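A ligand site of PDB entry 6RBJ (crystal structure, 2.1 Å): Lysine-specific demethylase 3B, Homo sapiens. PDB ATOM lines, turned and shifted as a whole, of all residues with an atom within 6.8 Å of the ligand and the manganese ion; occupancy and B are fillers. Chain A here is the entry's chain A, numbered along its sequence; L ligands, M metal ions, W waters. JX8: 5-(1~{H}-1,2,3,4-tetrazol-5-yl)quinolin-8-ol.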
ATOM      1  N   LYS A 107      20.337 -21.883  -3.030  1.00  0.00           N
ATOM      2  CA  LYS A 107      20.717 -20.641  -3.684  1.00  0.00           C
ATOM      3  C   LYS A 107      20.038 -20.602  -5.047  1.00  0.00           C
ATOM      4  O   LYS A 107      20.071 -21.580  -5.793  1.00  0.00           O
ATOM      5  CB  LYS A 107      22.242 -20.550  -3.828  1.00  0.00           C
ATOM      6  CG  LYS A 107      22.734 -19.380  -4.662  1.00  0.00           C
ATOM      7  CD  LYS A 107      24.261 -19.203  -4.554  1.00  0.00           C
ATOM      8  CE  LYS A 107      25.025 -20.473  -4.869  1.00  0.00           C
ATOM      9  NZ  LYS A 107      26.506 -20.252  -4.872  1.00  0.00           N
ATOM     10  N   TYR A 164      21.231 -11.700  -6.167  1.00  0.00           N
ATOM     11  CA  TYR A 164      21.742 -12.891  -5.498  1.00  0.00           C
ATOM     12  C   TYR A 164      20.783 -13.258  -4.373  1.00  0.00           C
ATOM     13  O   TYR A 164      20.679 -12.536  -3.380  1.00  0.00           O
ATOM     14  CB  TYR A 164      23.152 -12.669  -4.976  1.00  0.00           C
ATOM     15  CG  TYR A 164      24.167 -12.340  -6.049  1.00  0.00           C
ATOM     16  CD1 TYR A 164      25.114 -11.338  -5.846  1.00  0.00           C
ATOM     17  CD2 TYR A 164      24.206 -13.034  -7.254  1.00  0.00           C
ATOM     18  CE1 TYR A 164      26.038 -11.026  -6.806  1.00  0.00           C
ATOM     19  CE2 TYR A 164      25.143 -12.726  -8.229  1.00  0.00           C
ATOM     20  CZ  TYR A 164      26.059 -11.715  -7.987  1.00  0.00           C
ATOM     21  OH  TYR A 164      27.008 -11.390  -8.930  1.00  0.00           O
ATOM     22  N   ASN A 165      20.071 -14.373  -4.535  1.00  0.00           N
ATOM     23  CA  ASN A 165      19.055 -14.811  -3.593  1.00  0.00           C
ATOM     24  C   ASN A 165      19.434 -16.187  -3.063  1.00  0.00           C
ATOM     25  O   ASN A 165      19.668 -17.117  -3.843  1.00  0.00           O
ATOM     26  CB  ASN A 165      17.679 -14.839  -4.261  1.00  0.00           C
ATOM     27  CG  ASN A 165      17.365 -13.556  -5.015  1.00  0.00           C
ATOM     28  OD1 ASN A 165      17.030 -12.540  -4.411  1.00  0.00           O
ATOM     29  ND2 ASN A 165      17.467 -13.592  -6.344  1.00  0.00           N
ATOM     30  N   ALA A 166      19.479 -16.322  -1.735  1.00  0.00           N
ATOM     31  CA  ALA A 166      19.790 -17.617  -1.148  1.00  0.00           C
ATOM     32  C   ALA A 166      19.221 -17.680   0.265  1.00  0.00           C
ATOM     33  O   ALA A 166      19.109 -16.664   0.940  1.00  0.00           O
ATOM     34  CB  ALA A 166      21.294 -17.886  -1.137  1.00  0.00           C
ATOM     35  N   THR A 179      27.700 -19.567   1.163  1.00  0.00           N
ATOM     36  CA  THR A 179      26.703 -19.265   0.136  1.00  0.00           C
ATOM     37  C   THR A 179      27.371 -19.079  -1.214  1.00  0.00           C
ATOM     38  O   THR A 179      26.933 -19.636  -2.229  1.00  0.00           O
ATOM     39  CB  THR A 179      25.915 -18.012   0.527  1.00  0.00           C
ATOM     40  OG1 THR A 179      25.303 -18.200   1.805  1.00  0.00           O
ATOM     41  CG2 THR A 179      24.834 -17.693  -0.518  1.00  0.00           C
ATOM     42  N   THR A 180      28.442 -18.302  -1.237  1.00  0.00           N
ATOM     43  CA  THR A 180      29.319 -18.179  -2.397  1.00  0.00           C
ATOM     44  C   THR A 180      30.737 -18.403  -1.922  1.00  0.00           C
ATOM     45  O   THR A 180      31.203 -17.723  -0.991  1.00  0.00           O
ATOM     46  CB  THR A 180      29.175 -16.800  -3.053  1.00  0.00           C
ATOM     47  OG1 THR A 180      27.870 -16.682  -3.621  1.00  0.00           O
ATOM     48  CG2 THR A 180      30.211 -16.592  -4.159  1.00  0.00           C
ATOM     49  N   HIS A 183      36.496 -16.626  -4.104  1.00  0.00           N
ATOM     50  CA  HIS A 183      36.907 -16.372  -5.477  1.00  0.00           C
ATOM     51  C   HIS A 183      37.311 -14.915  -5.568  1.00  0.00           C
ATOM     52  O   HIS A 183      37.179 -14.150  -4.607  1.00  0.00           O
ATOM     53  CB  HIS A 183      35.783 -16.710  -6.471  1.00  0.00           C
ATOM     54  CG  HIS A 183      34.658 -15.723  -6.477  1.00  0.00           C
ATOM     55  ND1 HIS A 183      33.760 -15.613  -5.437  1.00  0.00           N
ATOM     56  CD2 HIS A 183      34.295 -14.799  -7.394  1.00  0.00           C
ATOM     57  CE1 HIS A 183      32.891 -14.666  -5.724  1.00  0.00           C
ATOM     58  NE2 HIS A 183      33.184 -14.158  -6.912  1.00  0.00           N
ATOM     59  N   LEU A 184      37.815 -14.519  -6.733  1.00  0.00           N
ATOM     60  CA  LEU A 184      38.100 -13.123  -6.994  1.00  0.00           C
ATOM     61  C   LEU A 184      37.536 -12.725  -8.348  1.00  0.00           C
ATOM     62  O   LEU A 184      37.218 -13.580  -9.189  1.00  0.00           O
ATOM     63  CB  LEU A 184      39.600 -12.810  -6.924  1.00  0.00           C
ATOM     64  CG  LEU A 184      40.561 -13.416  -7.957  1.00  0.00           C
ATOM     65  CD1 LEU A 184      40.554 -12.676  -9.289  1.00  0.00           C
ATOM     66  CD2 LEU A 184      41.972 -13.433  -7.381  1.00  0.00           C
ATOM     67  N   ASP A 185      37.379 -11.418  -8.534  1.00  0.00           N
ATOM     68  CA  ASP A 185      36.860 -10.855  -9.775  1.00  0.00           C
ATOM     69  C   ASP A 185      37.835  -9.831 -10.315  1.00  0.00           C
ATOM     70  O   ASP A 185      38.589  -9.205  -9.559  1.00  0.00           O
ATOM     71  CB  ASP A 185      35.491 -10.246  -9.551  1.00  0.00           C
ATOM     72  CG  ASP A 185      34.457 -11.280  -9.223  1.00  0.00           C
ATOM     73  OD1 ASP A 185      34.321 -12.233 -10.015  1.00  0.00           O
ATOM     74  OD2 ASP A 185      33.797 -11.171  -8.165  1.00  0.00           O
ATOM     75  N   ALA A 189      33.208  -4.224  -7.591  1.00  0.00           N
ATOM     76  CA  ALA A 189      31.785  -4.481  -7.459  1.00  0.00           C
ATOM     77  C   ALA A 189      31.274  -3.842  -6.185  1.00  0.00           C
ATOM     78  O   ALA A 189      31.992  -3.707  -5.191  1.00  0.00           O
ATOM     79  CB  ALA A 189      31.473  -5.982  -7.453  1.00  0.00           C
ATOM     80  N   ASN A 191      27.843  -4.431  -3.666  1.00  0.00           N
ATOM     81  CA  ASN A 191      26.848  -5.444  -3.363  1.00  0.00           C
ATOM     82  C   ASN A 191      25.949  -4.909  -2.253  1.00  0.00           C
ATOM     83  O   ASN A 191      26.419  -4.654  -1.145  1.00  0.00           O
ATOM     84  CB  ASN A 191      27.534  -6.752  -2.932  1.00  0.00           C
ATOM     85  CG  ASN A 191      26.554  -7.857  -2.597  1.00  0.00           C
ATOM     86  OD1 ASN A 191      25.679  -7.700  -1.743  1.00  0.00           O
ATOM     87  ND2 ASN A 191      26.703  -8.985  -3.269  1.00  0.00           N
ATOM     88  N   ALA A 235      24.444 -11.339   6.105  1.00  0.00           N
ATOM     89  CA  ALA A 235      25.470 -12.244   5.602  1.00  0.00           C
ATOM     90  C   ALA A 235      26.807 -11.906   6.234  1.00  0.00           C
ATOM     91  O   ALA A 235      27.073 -10.761   6.621  1.00  0.00           O
ATOM     92  CB  ALA A 235      25.600 -12.156   4.073  1.00  0.00           C
ATOM     93  N   TRP A 237      30.767 -11.875   5.491  1.00  0.00           N
ATOM     94  CA  TRP A 237      31.781 -11.814   4.452  1.00  0.00           C
ATOM     95  C   TRP A 237      33.164 -11.982   5.054  1.00  0.00           C
ATOM     96  O   TRP A 237      33.439 -11.522   6.157  1.00  0.00           O
ATOM     97  CB  TRP A 237      31.759 -10.477   3.707  1.00  0.00           C
ATOM     98  CG  TRP A 237      30.537 -10.191   2.895  1.00  0.00           C
ATOM     99  CD1 TRP A 237      29.259 -10.041   3.346  1.00  0.00           C
ATOM    100  CD2 TRP A 237      30.494  -9.995   1.477  1.00  0.00           C
ATOM    101  NE1 TRP A 237      28.418  -9.757   2.290  1.00  0.00           N
ATOM    102  CE2 TRP A 237      29.149  -9.722   1.139  1.00  0.00           C
ATOM    103  CE3 TRP A 237      31.454 -10.016   0.466  1.00  0.00           C
ATOM    104  CZ2 TRP A 237      28.750  -9.486  -0.180  1.00  0.00           C
ATOM    105  CZ3 TRP A 237      31.055  -9.773  -0.841  1.00  0.00           C
ATOM    106  CH2 TRP A 237      29.712  -9.518  -1.148  1.00  0.00           C
ATOM    107  N   GLN A 273      36.790 -21.717  -7.285  1.00  0.00           N
ATOM    108  CA  GLN A 273      35.607 -21.320  -6.520  1.00  0.00           C
ATOM    109  C   GLN A 273      34.973 -22.522  -5.816  1.00  0.00           C
ATOM    110  O   GLN A 273      33.750 -22.684  -5.806  1.00  0.00           O
ATOM    111  CB  GLN A 273      34.593 -20.598  -7.411  1.00  0.00           C
ATOM    112  CG  GLN A 273      33.536 -19.816  -6.647  1.00  0.00           C
ATOM    113  CD  GLN A 273      32.763 -18.844  -7.522  1.00  0.00           C
ATOM    114  OE1 GLN A 273      33.328 -18.216  -8.420  1.00  0.00           O
ATOM    115  NE2 GLN A 273      31.456 -18.737  -7.277  1.00  0.00           N
ATOM    116  N   GLN A 298      27.235  -7.910   6.786  1.00  0.00           N
ATOM    117  CA  GLN A 298      26.434  -7.046   5.940  1.00  0.00           C
ATOM    118  C   GLN A 298      25.004  -7.045   6.473  1.00  0.00           C
ATOM    119  O   GLN A 298      24.322  -8.084   6.446  1.00  0.00           O
ATOM    120  CB  GLN A 298      26.485  -7.534   4.492  1.00  0.00           C
ATOM    121  CG  GLN A 298      25.777  -6.651   3.496  1.00  0.00           C
ATOM    122  CD  GLN A 298      25.814  -7.225   2.095  1.00  0.00           C
ATOM    123  OE1 GLN A 298      25.882  -8.443   1.908  1.00  0.00           O
ATOM    124  NE2 GLN A 298      25.758  -6.351   1.106  1.00  0.00           N
ATOM    125  N   ILE A 306      33.787  -4.196  -3.074  1.00  0.00           N
ATOM    126  CA  ILE A 306      34.774  -5.263  -3.171  1.00  0.00           C
ATOM    127  C   ILE A 306      35.827  -4.846  -4.195  1.00  0.00           C
ATOM    128  O   ILE A 306      35.493  -4.718  -5.374  1.00  0.00           O
ATOM    129  CB  ILE A 306      34.134  -6.594  -3.562  1.00  0.00           C
ATOM    130  CG1 ILE A 306      33.019  -6.963  -2.571  1.00  0.00           C
ATOM    131  CG2 ILE A 306      35.196  -7.695  -3.619  1.00  0.00           C
ATOM    132  CD1 ILE A 306      31.628  -6.999  -3.198  1.00  0.00           C
ATOM    133  N   HIS A 312      37.230 -13.173  -1.902  1.00  0.00           N
ATOM    134  CA  HIS A 312      36.126 -12.905  -0.981  1.00  0.00           C
ATOM    135  C   HIS A 312      35.144 -14.062  -1.022  1.00  0.00           C
ATOM    136  O   HIS A 312      35.010 -14.747  -2.042  1.00  0.00           O
ATOM    137  CB  HIS A 312      35.431 -11.587  -1.332  1.00  0.00           C
ATOM    138  CG  HIS A 312      34.888 -11.549  -2.718  1.00  0.00           C
ATOM    139  ND1 HIS A 312      35.672 -11.306  -3.823  1.00  0.00           N
ATOM    140  CD2 HIS A 312      33.625 -11.733  -3.185  1.00  0.00           C
ATOM    141  CE1 HIS A 312      34.932 -11.341  -4.908  1.00  0.00           C
ATOM    142  NE2 HIS A 312      33.677 -11.594  -4.555  1.00  0.00           N
ATOM    143  N   GLN A 313      34.474 -14.275   0.100  1.00  0.00           N
ATOM    144  CA  GLN A 313      33.477 -15.319   0.267  1.00  0.00           C
ATOM    145  C   GLN A 313      32.323 -14.769   1.084  1.00  0.00           C
ATOM    146  O   GLN A 313      32.483 -13.815   1.857  1.00  0.00           O
ATOM    147  CB  GLN A 313      34.075 -16.556   0.949  1.00  0.00           C
ATOM    148  CG  GLN A 313      34.645 -16.260   2.332  1.00  0.00           C
ATOM    149  CD  GLN A 313      35.316 -17.455   2.971  1.00  0.00           C
ATOM    150  OE1 GLN A 313      35.823 -18.345   2.292  1.00  0.00           O
ATOM    151  NE2 GLN A 313      35.315 -17.490   4.305  1.00  0.00           N
ATOM    152  N   VAL A 314      31.145 -15.375   0.921  1.00  0.00           N
ATOM    153  CA  VAL A 314      29.896 -14.896   1.512  1.00  0.00           C
ATOM    154  C   VAL A 314      29.191 -16.071   2.181  1.00  0.00           C
ATOM    155  O   VAL A 314      29.051 -17.142   1.593  1.00  0.00           O
ATOM    156  CB  VAL A 314      28.966 -14.270   0.452  1.00  0.00           C
ATOM    157  CG1 VAL A 314      27.713 -13.695   1.122  1.00  0.00           C
ATOM    158  CG2 VAL A 314      29.682 -13.196  -0.327  1.00  0.00           C
ATOM    159  N   ASN A 316      25.569 -16.619   4.156  1.00  0.00           N
ATOM    160  CA  ASN A 316      24.284 -16.051   4.557  1.00  0.00           C
ATOM    161  C   ASN A 316      23.909 -16.516   5.954  1.00  0.00           C
ATOM    162  O   ASN A 316      23.899 -17.716   6.244  1.00  0.00           O
ATOM    163  CB  ASN A 316      23.194 -16.451   3.565  1.00  0.00           C
ATOM    164  CG  ASN A 316      23.134 -15.522   2.367  1.00  0.00           C
ATOM    165  OD1 ASN A 316      24.012 -14.688   2.169  1.00  0.00           O
ATOM    166  ND2 ASN A 316      22.099 -15.685   1.558  1.00  0.00           N
ATOM    167  N   CYS A 320      18.550 -13.931   2.309  1.00  0.00           N
ATOM    168  CA  CYS A 320      18.936 -12.610   1.835  1.00  0.00           C
ATOM    169  C   CYS A 320      18.554 -12.394   0.379  1.00  0.00           C
ATOM    170  O   CYS A 320      18.549 -13.330  -0.431  1.00  0.00           O
ATOM    171  CB  CYS A 320      20.453 -12.383   1.924  1.00  0.00           C
ATOM    172  SG  CYS A 320      21.124 -12.453   3.559  1.00  0.00           S
ATOM    173  N   LYS A 322      20.248  -9.815  -2.334  1.00  0.00           N
ATOM    174  CA  LYS A 322      21.299  -8.856  -2.607  1.00  0.00           C
ATOM    175  C   LYS A 322      21.281  -8.491  -4.082  1.00  0.00           C
ATOM    176  O   LYS A 322      20.876  -9.290  -4.926  1.00  0.00           O
ATOM    177  CB  LYS A 322      22.674  -9.417  -2.232  1.00  0.00           C
ATOM    178  CG  LYS A 322      22.717 -10.087  -0.874  1.00  0.00           C
ATOM    179  CD  LYS A 322      24.138 -10.413  -0.464  1.00  0.00           C
ATOM    180  CE  LYS A 322      24.191 -11.437   0.646  1.00  0.00           C
ATOM    181  NZ  LYS A 322      23.870 -12.815   0.178  1.00  0.00           N
ATOM    182  N   ALA A 324      23.972  -6.654  -6.932  1.00  0.00           N
ATOM    183  CA  ALA A 324      25.358  -6.265  -7.137  1.00  0.00           C
ATOM    184  C   ALA A 324      25.534  -5.662  -8.514  1.00  0.00           C
ATOM    185  O   ALA A 324      24.868  -6.059  -9.472  1.00  0.00           O
ATOM    186  CB  ALA A 324      26.295  -7.466  -6.972  1.00  0.00           C
ATOM    187  N   ASP A 326      28.834  -4.386 -11.137  1.00  0.00           N
ATOM    188  CA  ASP A 326      30.251  -4.283 -11.419  1.00  0.00           C
ATOM    189  C   ASP A 326      30.598  -2.883 -11.942  1.00  0.00           C
ATOM    190  O   ASP A 326      29.772  -2.204 -12.560  1.00  0.00           O
ATOM    191  CB  ASP A 326      30.675  -5.305 -12.455  1.00  0.00           C
ATOM    192  CG  ASP A 326      30.669  -6.728 -11.920  1.00  0.00           C
ATOM    193  OD1 ASP A 326      30.665  -6.918 -10.681  1.00  0.00           O
ATOM    194  OD2 ASP A 326      30.676  -7.668 -12.745  1.00  0.00           O
HETATM  195  N1  JX8 L   1      25.258 -12.959  -2.030  1.00  0.00           N
HETATM  196  N3  JX8 L   1      26.308 -14.311  -3.250  1.00  0.00           N
HETATM  197  C4  JX8 L   1      28.091 -12.814  -4.194  1.00  0.00           C
HETATM  198  C5  JX8 L   1      26.885 -13.122  -3.403  1.00  0.00           C
HETATM  199  C6  JX8 L   1      27.550 -14.309  -6.146  1.00  0.00           C
HETATM  200  C7  JX8 L   1      27.905 -14.777  -7.374  1.00  0.00           C
HETATM  201  C8  JX8 L   1      29.084 -14.317  -7.950  1.00  0.00           C
HETATM  202  N   JX8 L   1      26.226 -12.253  -2.658  1.00  0.00           N
HETATM  203  C   JX8 L   1      30.089 -11.466  -4.344  1.00  0.00           C
HETATM  204  O   JX8 L   1      31.423 -11.501  -6.297  1.00  0.00           O
HETATM  205  C1  JX8 L   1      30.371 -11.962  -5.583  1.00  0.00           C
HETATM  206  C2  JX8 L   1      29.530 -12.951  -6.171  1.00  0.00           C
HETATM  207  C3  JX8 L   1      28.368 -13.371  -5.475  1.00  0.00           C
HETATM  208  C9  JX8 L   1      28.967 -11.892  -3.654  1.00  0.00           C
HETATM  209  N2  JX8 L   1      25.296 -14.204  -2.363  1.00  0.00           N
HETATM  210  N4  JX8 L   1      29.883 -13.433  -7.397  1.00  0.00           N
HETATM  211 MN    MN M   1      32.001 -12.637  -7.934  1.00  0.00          MN
HETATM  212  O   HOH W   1      23.043 -15.687  -2.924  1.00  0.00           O
HETATM  213  O   HOH W   2      29.029  -8.827  -5.484  1.00  0.00           O
HETATM  214  O   HOH W   3      30.973 -11.131  -8.960  1.00  0.00           O
HETATM  215  O   HOH W   4      32.069 -13.815  -9.715  1.00  0.00           O
HETATM  216  O   HOH W   5      33.290  -8.796  -7.087  1.00  0.00           O
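Tyr 164 touches the ligand.
Thr 179 touches the ligand.
CH2 of Trp 237 touches C9 of the ligand, at 3.5 Å.
Val 314 touches the ligand (CG2 to C9, 3.6 Å).
Hydrophobic or aromatic side chains that line the ligand: Tyr 164, His 183, Trp 237, His 312 and Val 314.
Within 4 Å of the ligand: Tyr 164, Thr 179, Thr 180, His 183, Asp 185, Asn 191, Trp 237, His 312, Val 314 and Lys 322.
O of His 183 lies within hydrogen-bond range of N of His 312 (2.9 Å).
O of Lys 322 sits at hydrogen-bond distance from N of Tyr 164 (2.7 Å).
OD1 of Asn 316 lies within hydrogen-bond range of NZ of Lys 322, 2.7 Å away.
N of Val 314 sits at hydrogen-bond distance from O of Thr 180 (3.0 Å).
The side-chain amide nitrogen of Gln 298 lies within hydrogen-bond range of the backbone carbonyl oxygen of Asn 191, 2.9 Å away.
NE1 of Trp 237 sits at hydrogen-bond distance from OE1 of Gln 298 (2.9 Å).
O of Val 314 lies within hydrogen-bond range of N of Thr 179 (2.8 Å).
OG1 of Thr 179 is in hydrogen-bond range of N of Asn 316 (2.8 Å).
Merely in contact with the manganese ion: His 312.
The manganese ion is bound by O of the ligand (2.1 Å).
Water W3 is bound to the manganese ion.
The manganese ion is bound by water W4, 2.1 Å away.
NE2 of His 183 binds the manganese ion, 2.2 Å away.
N4 of the ligand binds the manganese ion (2.3 Å).
OD2 of Asp 185 is bound to the manganese ion (2.3 Å).
The manganese ion has six donor atoms within binding distance.
A nitrogen (N1) of the ligand lies within hydrogen-bond range of the side-chain amino group (NZ) of Lys 322.
A ring nitrogen (NE2) of His 312 lies close to an oxygen (O) of the ligand, 2.9 Å away.
The side-chain hydroxyl (OG1) of Thr 180 sits at hydrogen-bond distance from a nitrogen (N3) of the ligand (2.9 Å).
ND2 of Asn 191 is in hydrogen-bond range of N of the ligand (3.4 Å).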
